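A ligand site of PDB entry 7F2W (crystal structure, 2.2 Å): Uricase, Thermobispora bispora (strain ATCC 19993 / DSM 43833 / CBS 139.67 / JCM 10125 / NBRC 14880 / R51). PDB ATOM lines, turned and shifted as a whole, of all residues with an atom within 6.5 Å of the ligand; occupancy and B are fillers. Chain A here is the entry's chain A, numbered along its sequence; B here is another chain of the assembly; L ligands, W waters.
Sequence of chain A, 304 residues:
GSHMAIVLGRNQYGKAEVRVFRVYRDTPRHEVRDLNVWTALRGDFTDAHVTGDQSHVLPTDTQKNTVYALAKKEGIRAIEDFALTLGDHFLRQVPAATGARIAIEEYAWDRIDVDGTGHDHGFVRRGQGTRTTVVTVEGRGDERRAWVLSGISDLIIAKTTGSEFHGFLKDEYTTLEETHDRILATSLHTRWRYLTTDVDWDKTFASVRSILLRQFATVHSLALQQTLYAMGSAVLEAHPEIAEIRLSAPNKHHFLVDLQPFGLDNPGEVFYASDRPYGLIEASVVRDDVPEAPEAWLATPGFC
O1 of the ligand is in hydrogen-bond range of N of Leu 224 (2.6 Å).
An oxygen (O1) of the ligand lies within hydrogen-bond range of the guanidinium group (NH1) of Arg 182 (2.8 Å).
The side-chain amide oxygen (OE1) of Gln 225 lies within hydrogen-bond range of a nitrogen (N1) of the ligand.
N of Thr 60 of chain B is in hydrogen-bond range of O3 of the ligand, at 3.4 Å.
N4 of the ligand sits at hydrogen-bond distance from OG1 of Thr 60 of chain B (3.0 Å).
N of Asp 61 of chain B sits at hydrogen-bond distance from O3 of the ligand (2.9 Å).
A nitrogen (N2) of the ligand lies close to the side-chain amide nitrogen (ND2) of Asn 251 (3.4 Å).
OG of Ser 163 is in hydrogen-bond range of NE of Arg 182.
OG1 of Thr 60 of chain B is in hydrogen-bond range of NZ of Lys 15 of chain B, 3.0 Å away.
O of Ala 223 lies within hydrogen-bond range of OG of Ser 221, at 3.0 Å.
The backbone carbonyl oxygen (O) of Asn 251 lies within hydrogen-bond range of a ring nitrogen (NE2) of His 253 (3.4 Å).
The backbone NH (N) of Asn 251 lies within hydrogen-bond range of the backbone carbonyl oxygen (O) of Gly 279, at 2.8 Å.
The side-chain hydroxyl of Tyr 13 of chain B lies within hydrogen-bond range of the backbone carbonyl oxygen of Leu 58 of chain B (2.6 Å).
CZ of Phe 165 touches C4 of the ligand (3.4 Å).
Leu 176 touches the ligand (CD2 to O3, 3.6 Å).
Ala 223 touches the ligand (CA to O1, 3.4 Å).
Tyr 13 of chain B touches the ligand.
Val 57 of chain B touches the ligand (CG1 to O2, 3.8 Å).
Pro 59 of chain B touches the ligand.
Hydrophobic or aromatic side chains that line the ligand: Phe 165, Leu 176, Ala 223, Leu 224, Tyr 13 of chain B, Val 57 of chain B and Pro 59 of chain B.
Within 4 Å of the ligand: Phe 165, Leu 176, Arg 182, Ala 223, Leu 224, Gln 225, Asn 251, Tyr 13 of chain B, Val 57 of chain B, Pro 59 of chain B, Thr 60 of chain B and Asp 61 of chain B.
The nearest printed residue that does not touch the ligand is Ile 281 (4.3 Å).
Water W1 lies within hydrogen-bond range of the side-chain hydroxyl (OG1) of Thr 60 of chain B (2.9 Å), the side-chain amide nitrogen (ND2) of Asn 251 (3.1 Å) and a nitrogen (N3) of the ligand (3.4 Å).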
ATOM      1  N   SER A 163     -28.835   6.439  -4.493  1.00  0.00           N
ATOM      2  CA  SER A 163     -27.855   6.613  -5.553  1.00  0.00           C
ATOM      3  C   SER A 163     -28.591   6.830  -6.871  1.00  0.00           C
ATOM      4  O   SER A 163     -29.398   5.977  -7.275  1.00  0.00           O
ATOM      5  CB  SER A 163     -26.918   5.411  -5.659  1.00  0.00           C
ATOM      6  OG  SER A 163     -26.057   5.516  -6.795  1.00  0.00           O
ATOM      7  N   GLU A 164     -28.317   7.946  -7.522  1.00  0.00           N
ATOM      8  CA  GLU A 164     -28.930   8.332  -8.778  1.00  0.00           C
ATOM      9  C   GLU A 164     -27.853   8.571  -9.821  1.00  0.00           C
ATOM     10  O   GLU A 164     -26.675   8.727  -9.494  1.00  0.00           O
ATOM     11  CB  GLU A 164     -29.746   9.634  -8.628  1.00  0.00           C
ATOM     12  CG  GLU A 164     -30.788   9.578  -7.548  1.00  0.00           C
ATOM     13  CD  GLU A 164     -31.610  10.861  -7.472  1.00  0.00           C
ATOM     14  OE1 GLU A 164     -31.857  11.500  -8.515  1.00  0.00           O
ATOM     15  OE2 GLU A 164     -32.017  11.216  -6.343  1.00  0.00           O
ATOM     16  N   PHE A 165     -28.284   8.621 -11.087  1.00  0.00           N
ATOM     17  CA  PHE A 165     -27.412   9.034 -12.190  1.00  0.00           C
ATOM     18  C   PHE A 165     -28.314   9.379 -13.373  1.00  0.00           C
ATOM     19  O   PHE A 165     -28.840   8.486 -14.037  1.00  0.00           O
ATOM     20  CB  PHE A 165     -26.389   7.957 -12.558  1.00  0.00           C
ATOM     21  CG  PHE A 165     -25.322   8.444 -13.511  1.00  0.00           C
ATOM     22  CD1 PHE A 165     -24.503   9.515 -13.162  1.00  0.00           C
ATOM     23  CD2 PHE A 165     -25.129   7.821 -14.738  1.00  0.00           C
ATOM     24  CE1 PHE A 165     -23.519   9.973 -14.026  1.00  0.00           C
ATOM     25  CE2 PHE A 165     -24.134   8.261 -15.607  1.00  0.00           C
ATOM     26  CZ  PHE A 165     -23.339   9.347 -15.251  1.00  0.00           C
ATOM     27  N   LEU A 176     -27.384   4.115 -22.109  1.00  0.00           N
ATOM     28  CA  LEU A 176     -27.662   4.022 -20.681  1.00  0.00           C
ATOM     29  C   LEU A 176     -28.958   4.755 -20.337  1.00  0.00           C
ATOM     30  O   LEU A 176     -29.092   5.957 -20.619  1.00  0.00           O
ATOM     31  CB  LEU A 176     -26.490   4.599 -19.889  1.00  0.00           C
ATOM     32  CG  LEU A 176     -26.684   4.609 -18.373  1.00  0.00           C
ATOM     33  CD1 LEU A 176     -26.932   3.189 -17.895  1.00  0.00           C
ATOM     34  CD2 LEU A 176     -25.465   5.238 -17.681  1.00  0.00           C
ATOM     35  N   ARG A 182     -30.390   3.143  -7.959  1.00  0.00           N
ATOM     36  CA  ARG A 182     -29.499   2.076  -8.360  1.00  0.00           C
ATOM     37  C   ARG A 182     -28.633   1.706  -7.164  1.00  0.00           C
ATOM     38  O   ARG A 182     -28.626   2.381  -6.136  1.00  0.00           O
ATOM     39  CB  ARG A 182     -28.611   2.492  -9.547  1.00  0.00           C
ATOM     40  CG  ARG A 182     -27.603   3.560  -9.119  1.00  0.00           C
ATOM     41  CD  ARG A 182     -26.720   4.061 -10.253  1.00  0.00           C
ATOM     42  NE  ARG A 182     -25.730   5.006  -9.753  1.00  0.00           N
ATOM     43  CZ  ARG A 182     -24.694   5.470 -10.447  1.00  0.00           C
ATOM     44  NH1 ARG A 182     -23.850   6.323  -9.889  1.00  0.00           N
ATOM     45  NH2 ARG A 182     -24.524   5.079 -11.703  1.00  0.00           N
ATOM     46  N   LEU A 184     -24.898   1.428  -5.680  1.00  0.00           N
ATOM     47  CA  LEU A 184     -23.572   2.031  -5.817  1.00  0.00           C
ATOM     48  C   LEU A 184     -22.599   1.224  -4.966  1.00  0.00           C
ATOM     49  O   LEU A 184     -22.607   1.347  -3.745  1.00  0.00           O
ATOM     50  CB  LEU A 184     -23.603   3.481  -5.376  1.00  0.00           C
ATOM     51  CG  LEU A 184     -22.247   4.163  -5.480  1.00  0.00           C
ATOM     52  CD1 LEU A 184     -21.738   4.087  -6.910  1.00  0.00           C
ATOM     53  CD2 LEU A 184     -22.344   5.599  -5.013  1.00  0.00           C
ATOM     54  N   SER A 221     -26.477  10.245  -3.397  1.00  0.00           N
ATOM     55  CA  SER A 221     -25.486  10.310  -4.466  1.00  0.00           C
ATOM     56  C   SER A 221     -26.157  10.609  -5.809  1.00  0.00           C
ATOM     57  O   SER A 221     -27.064   9.886  -6.225  1.00  0.00           O
ATOM     58  CB  SER A 221     -24.699   9.013  -4.549  1.00  0.00           C
ATOM     59  OG  SER A 221     -23.725   9.083  -5.570  1.00  0.00           O
ATOM     60  N   LEU A 222     -25.704  11.672  -6.478  1.00  0.00           N
ATOM     61  CA  LEU A 222     -26.113  11.968  -7.844  1.00  0.00           C
ATOM     62  C   LEU A 222     -25.114  11.451  -8.865  1.00  0.00           C
ATOM     63  O   LEU A 222     -25.377  11.509 -10.075  1.00  0.00           O
ATOM     64  CB  LEU A 222     -26.321  13.475  -8.031  1.00  0.00           C
ATOM     65  CG  LEU A 222     -27.330  14.118  -7.073  1.00  0.00           C
ATOM     66  CD1 LEU A 222     -27.471  15.611  -7.318  1.00  0.00           C
ATOM     67  CD2 LEU A 222     -28.694  13.451  -7.205  1.00  0.00           C
ATOM     68  N   ALA A 223     -23.981  10.907  -8.397  1.00  0.00           N
ATOM     69  CA  ALA A 223     -22.962  10.278  -9.211  1.00  0.00           C
ATOM     70  C   ALA A 223     -21.833   9.831  -8.298  1.00  0.00           C
ATOM     71  O   ALA A 223     -21.639  10.403  -7.219  1.00  0.00           O
ATOM     72  CB  ALA A 223     -22.409  11.229 -10.293  1.00  0.00           C
ATOM     73  N   LEU A 224     -21.053   8.823  -8.712  1.00  0.00           N
ATOM     74  CA  LEU A 224     -19.893   8.462  -7.902  1.00  0.00           C
ATOM     75  C   LEU A 224     -18.935   9.652  -7.766  1.00  0.00           C
ATOM     76  O   LEU A 224     -18.337   9.856  -6.700  1.00  0.00           O
ATOM     77  CB  LEU A 224     -19.192   7.244  -8.502  1.00  0.00           C
ATOM     78  CG  LEU A 224     -18.022   6.617  -7.710  1.00  0.00           C
ATOM     79  CD1 LEU A 224     -18.375   6.451  -6.217  1.00  0.00           C
ATOM     80  CD2 LEU A 224     -17.617   5.278  -8.324  1.00  0.00           C
ATOM     81  N   GLN A 225     -18.800  10.464  -8.823  1.00  0.00           N
ATOM     82  CA  GLN A 225     -17.992  11.683  -8.762  1.00  0.00           C
ATOM     83  C   GLN A 225     -18.403  12.547  -7.573  1.00  0.00           C
ATOM     84  O   GLN A 225     -17.564  13.028  -6.806  1.00  0.00           O
ATOM     85  CB  GLN A 225     -18.153  12.487 -10.055  1.00  0.00           C
ATOM     86  CG  GLN A 225     -17.456  11.890 -11.265  1.00  0.00           C
ATOM     87  CD  GLN A 225     -18.323  10.910 -12.038  1.00  0.00           C
ATOM     88  OE1 GLN A 225     -19.101  10.160 -11.462  1.00  0.00           O
ATOM     89  NE2 GLN A 225     -18.167  10.897 -13.373  1.00  0.00           N
ATOM     90  N   ASN A 251     -16.631   1.638  -9.994  1.00  0.00           N
ATOM     91  CA  ASN A 251     -18.081   1.494  -9.946  1.00  0.00           C
ATOM     92  C   ASN A 251     -18.346   0.063 -10.362  1.00  0.00           C
ATOM     93  O   ASN A 251     -18.418  -0.256 -11.548  1.00  0.00           O
ATOM     94  CB  ASN A 251     -18.783   2.503 -10.872  1.00  0.00           C
ATOM     95  CG  ASN A 251     -20.262   2.673 -10.548  1.00  0.00           C
ATOM     96  OD1 ASN A 251     -20.825   1.962  -9.691  1.00  0.00           O
ATOM     97  ND2 ASN A 251     -20.919   3.613 -11.234  1.00  0.00           N
ATOM     98  N   HIS A 253     -20.455  -2.528 -11.200  1.00  0.00           N
ATOM     99  CA  HIS A 253     -21.840  -2.484 -11.613  1.00  0.00           C
ATOM    100  C   HIS A 253     -22.611  -3.702 -11.110  1.00  0.00           C
ATOM    101  O   HIS A 253     -22.163  -4.838 -11.288  1.00  0.00           O
ATOM    102  CB  HIS A 253     -21.924  -2.409 -13.132  1.00  0.00           C
ATOM    103  CG  HIS A 253     -21.143  -1.272 -13.696  1.00  0.00           C
ATOM    104  ND1 HIS A 253     -21.454   0.049 -13.435  1.00  0.00           N
ATOM    105  CD2 HIS A 253     -20.028  -1.245 -14.475  1.00  0.00           C
ATOM    106  CE1 HIS A 253     -20.588   0.835 -14.049  1.00  0.00           C
ATOM    107  NE2 HIS A 253     -19.715   0.068 -14.682  1.00  0.00           N
ATOM    108  N   GLY A 279     -16.655   1.139 -14.185  1.00  0.00           N
ATOM    109  CA  GLY A 279     -16.289   2.539 -14.140  1.00  0.00           C
ATOM    110  C   GLY A 279     -15.123   2.730 -13.177  1.00  0.00           C
ATOM    111  O   GLY A 279     -14.961   1.997 -12.216  1.00  0.00           O
ATOM    112  N   ILE A 281     -13.690   6.043 -11.283  1.00  0.00           N
ATOM    113  CA  ILE A 281     -13.905   7.468 -11.035  1.00  0.00           C
ATOM    114  C   ILE A 281     -12.880   7.889 -10.005  1.00  0.00           C
ATOM    115  O   ILE A 281     -12.803   7.313  -8.916  1.00  0.00           O
ATOM    116  CB  ILE A 281     -15.343   7.751 -10.549  1.00  0.00           C
ATOM    117  CG1 ILE A 281     -16.318   7.828 -11.728  1.00  0.00           C
ATOM    118  CG2 ILE A 281     -15.409   9.067  -9.817  1.00  0.00           C
ATOM    119  CD1 ILE A 281     -16.606   6.516 -12.362  1.00  0.00           C
ATOM    120  N   TYR B  13     -12.041  10.242 -15.090  1.00  0.00           N
ATOM    121  CA  TYR B  13     -13.009   9.158 -14.964  1.00  0.00           C
ATOM    122  C   TYR B  13     -13.168   8.485 -16.326  1.00  0.00           C
ATOM    123  O   TYR B  13     -12.914   9.088 -17.368  1.00  0.00           O
ATOM    124  CB  TYR B  13     -14.365   9.669 -14.488  1.00  0.00           C
ATOM    125  CG  TYR B  13     -15.197  10.171 -15.641  1.00  0.00           C
ATOM    126  CD1 TYR B  13     -14.817  11.320 -16.320  1.00  0.00           C
ATOM    127  CD2 TYR B  13     -16.321   9.483 -16.079  1.00  0.00           C
ATOM    128  CE1 TYR B  13     -15.548  11.784 -17.397  1.00  0.00           C
ATOM    129  CE2 TYR B  13     -17.057   9.942 -17.149  1.00  0.00           C
ATOM    130  CZ  TYR B  13     -16.663  11.105 -17.807  1.00  0.00           C
ATOM    131  OH  TYR B  13     -17.382  11.581 -18.882  1.00  0.00           O
ATOM    132  N   GLY B  14     -13.608   7.232 -16.283  1.00  0.00           N
ATOM    133  CA  GLY B  14     -13.852   6.499 -17.522  1.00  0.00           C
ATOM    134  C   GLY B  14     -14.163   5.052 -17.221  1.00  0.00           C
ATOM    135  O   GLY B  14     -14.405   4.671 -16.076  1.00  0.00           O
ATOM    136  N   LYS B  15     -14.156   4.242 -18.273  1.00  0.00           N
ATOM    137  CA  LYS B  15     -14.390   2.807 -18.135  1.00  0.00           C
ATOM    138  C   LYS B  15     -13.069   2.060 -18.076  1.00  0.00           C
ATOM    139  O   LYS B  15     -12.196   2.284 -18.925  1.00  0.00           O
ATOM    140  CB  LYS B  15     -15.239   2.258 -19.278  1.00  0.00           C
ATOM    141  CG  LYS B  15     -15.759   0.845 -18.994  1.00  0.00           C
ATOM    142  CD  LYS B  15     -16.792   0.829 -17.838  1.00  0.00           C
ATOM    143  CE  LYS B  15     -18.192   1.053 -18.351  1.00  0.00           C
ATOM    144  NZ  LYS B  15     -19.168   1.230 -17.234  1.00  0.00           N
ATOM    145  N   GLN B  54     -24.668  16.490 -13.894  1.00  0.00           N
ATOM    146  CA  GLN B  54     -23.947  15.589 -14.785  1.00  0.00           C
ATOM    147  C   GLN B  54     -23.984  16.016 -16.257  1.00  0.00           C
ATOM    148  O   GLN B  54     -23.601  15.221 -17.124  1.00  0.00           O
ATOM    149  CB  GLN B  54     -24.487  14.172 -14.644  1.00  0.00           C
ATOM    150  CG  GLN B  54     -24.512  13.624 -13.201  1.00  0.00           C
ATOM    151  CD  GLN B  54     -23.161  13.761 -12.521  1.00  0.00           C
ATOM    152  OE1 GLN B  54     -23.032  14.378 -11.458  1.00  0.00           O
ATOM    153  NE2 GLN B  54     -22.144  13.175 -13.124  1.00  0.00           N
ATOM    154  N   VAL B  57     -20.977  15.172 -18.367  1.00  0.00           N
ATOM    155  CA  VAL B  57     -20.369  13.855 -18.198  1.00  0.00           C
ATOM    156  C   VAL B  57     -20.916  12.922 -19.271  1.00  0.00           C
ATOM    157  O   VAL B  57     -22.119  12.669 -19.331  1.00  0.00           O
ATOM    158  CB  VAL B  57     -20.656  13.299 -16.795  1.00  0.00           C
ATOM    159  CG1 VAL B  57     -20.128  11.864 -16.666  1.00  0.00           C
ATOM    160  CG2 VAL B  57     -20.019  14.191 -15.727  1.00  0.00           C
ATOM    161  N   LEU B  58     -20.031  12.446 -20.150  1.00  0.00           N
ATOM    162  CA  LEU B  58     -20.387  11.320 -20.989  1.00  0.00           C
ATOM    163  C   LEU B  58     -20.260  10.045 -20.169  1.00  0.00           C
ATOM    164  O   LEU B  58     -19.169   9.778 -19.627  1.00  0.00           O
ATOM    165  CB  LEU B  58     -19.507  11.254 -22.228  1.00  0.00           C
ATOM    166  CG  LEU B  58     -19.901  10.192 -23.277  1.00  0.00           C
ATOM    167  CD1 LEU B  58     -21.089  10.623 -24.117  1.00  0.00           C
ATOM    168  CD2 LEU B  58     -18.730   9.876 -24.192  1.00  0.00           C
ATOM    169  N   PRO B  59     -21.311   9.246 -20.036  1.00  0.00           N
ATOM    170  CA  PRO B  59     -21.273   8.095 -19.111  1.00  0.00           C
ATOM    171  C   PRO B  59     -20.162   7.114 -19.478  1.00  0.00           C
ATOM    172  O   PRO B  59     -19.868   6.895 -20.654  1.00  0.00           O
ATOM    173  CB  PRO B  59     -22.658   7.467 -19.275  1.00  0.00           C
ATOM    174  CG  PRO B  59     -23.527   8.560 -19.842  1.00  0.00           C
ATOM    175  CD  PRO B  59     -22.608   9.359 -20.733  1.00  0.00           C
ATOM    176  N   THR B  60     -19.560   6.523 -18.440  1.00  0.00           N
ATOM    177  CA  THR B  60     -18.555   5.482 -18.669  1.00  0.00           C
ATOM    178  C   THR B  60     -19.133   4.338 -19.499  1.00  0.00           C
ATOM    179  O   THR B  60     -18.413   3.695 -20.272  1.00  0.00           O
ATOM    180  CB  THR B  60     -17.998   4.944 -17.346  1.00  0.00           C
ATOM    181  OG1 THR B  60     -19.004   4.194 -16.668  1.00  0.00           O
ATOM    182  CG2 THR B  60     -17.486   6.077 -16.431  1.00  0.00           C
ATOM    183  N   ASP B  61     -20.437   4.052 -19.343  1.00  0.00           N
ATOM    184  CA  ASP B  61     -21.085   3.027 -20.158  1.00  0.00           C
ATOM    185  C   ASP B  61     -21.000   3.365 -21.644  1.00  0.00           C
ATOM    186  O   ASP B  61     -20.804   2.479 -22.483  1.00  0.00           O
ATOM    187  CB  ASP B  61     -22.545   2.872 -19.745  1.00  0.00           C
ATOM    188  CG  ASP B  61     -23.216   1.672 -20.398  1.00  0.00           C
ATOM    189  OD1 ASP B  61     -22.918   0.544 -19.974  1.00  0.00           O
ATOM    190  OD2 ASP B  61     -24.022   1.860 -21.336  1.00  0.00           O
ATOM    191  N   THR B  62     -21.168   4.642 -21.985  1.00  0.00           N
ATOM    192  CA  THR B  62     -21.017   5.067 -23.378  1.00  0.00           C
ATOM    193  C   THR B  62     -19.584   4.877 -23.847  1.00  0.00           C
ATOM    194  O   THR B  62     -19.331   4.482 -24.989  1.00  0.00           O
ATOM    195  CB  THR B  62     -21.445   6.530 -23.529  1.00  0.00           C
ATOM    196  OG1 THR B  62     -22.831   6.653 -23.155  1.00  0.00           O
ATOM    197  CG2 THR B  62     -21.256   7.010 -24.969  1.00  0.00           C
ATOM    198  N   GLN B  63     -18.618   5.149 -22.961  1.00  0.00           N
ATOM    199  CA  GLN B  63     -17.216   4.992 -23.331  1.00  0.00           C
ATOM    200  C   GLN B  63     -16.919   3.528 -23.629  1.00  0.00           C
ATOM    201  O   GLN B  63     -16.179   3.216 -24.573  1.00  0.00           O
ATOM    202  CB  GLN B  63     -16.308   5.547 -22.224  1.00  0.00           C
ATOM    203  CG  GLN B  63     -16.553   7.022 -21.951  1.00  0.00           C
ATOM    204  CD  GLN B  63     -15.706   7.579 -20.802  1.00  0.00           C
ATOM    205  OE1 GLN B  63     -14.495   7.327 -20.728  1.00  0.00           O
ATOM    206  NE2 GLN B  63     -16.342   8.336 -19.919  1.00  0.00           N
HETATM  207  N1  LIG L   1     -20.589   8.236 -12.835  1.00  0.00           N
HETATM  208  C1  LIG L   1     -21.487   7.472 -12.144  1.00  0.00           C
HETATM  209  C2  LIG L   1     -20.347   7.954 -14.119  1.00  0.00           C
HETATM  210  N2  LIG L   1     -22.110   6.438 -12.749  1.00  0.00           N
HETATM  211  O1  LIG L   1     -21.726   7.685 -11.003  1.00  0.00           O
HETATM  212  C3  LIG L   1     -21.880   6.144 -14.037  1.00  0.00           C
HETATM  213  C4  LIG L   1     -21.008   6.893 -14.728  1.00  0.00           C
HETATM  214  N3  LIG L   1     -22.391   5.173 -14.827  1.00  0.00           N
HETATM  215  O2  LIG L   1     -19.563   8.619 -14.749  1.00  0.00           O
HETATM  216  N4  LIG L   1     -20.968   6.386 -15.960  1.00  0.00           N
HETATM  217  C5  LIG L   1     -21.815   5.326 -16.026  1.00  0.00           C
HETATM  218  O3  LIG L   1     -22.017   4.641 -16.989  1.00  0.00           O
HETATM  219  O   HOH W   1     -19.240   4.317 -13.780  1.00  0.00           O
HETATM  220  O   HOH W   2     -24.143   2.861 -14.511  1.00  0.00           O
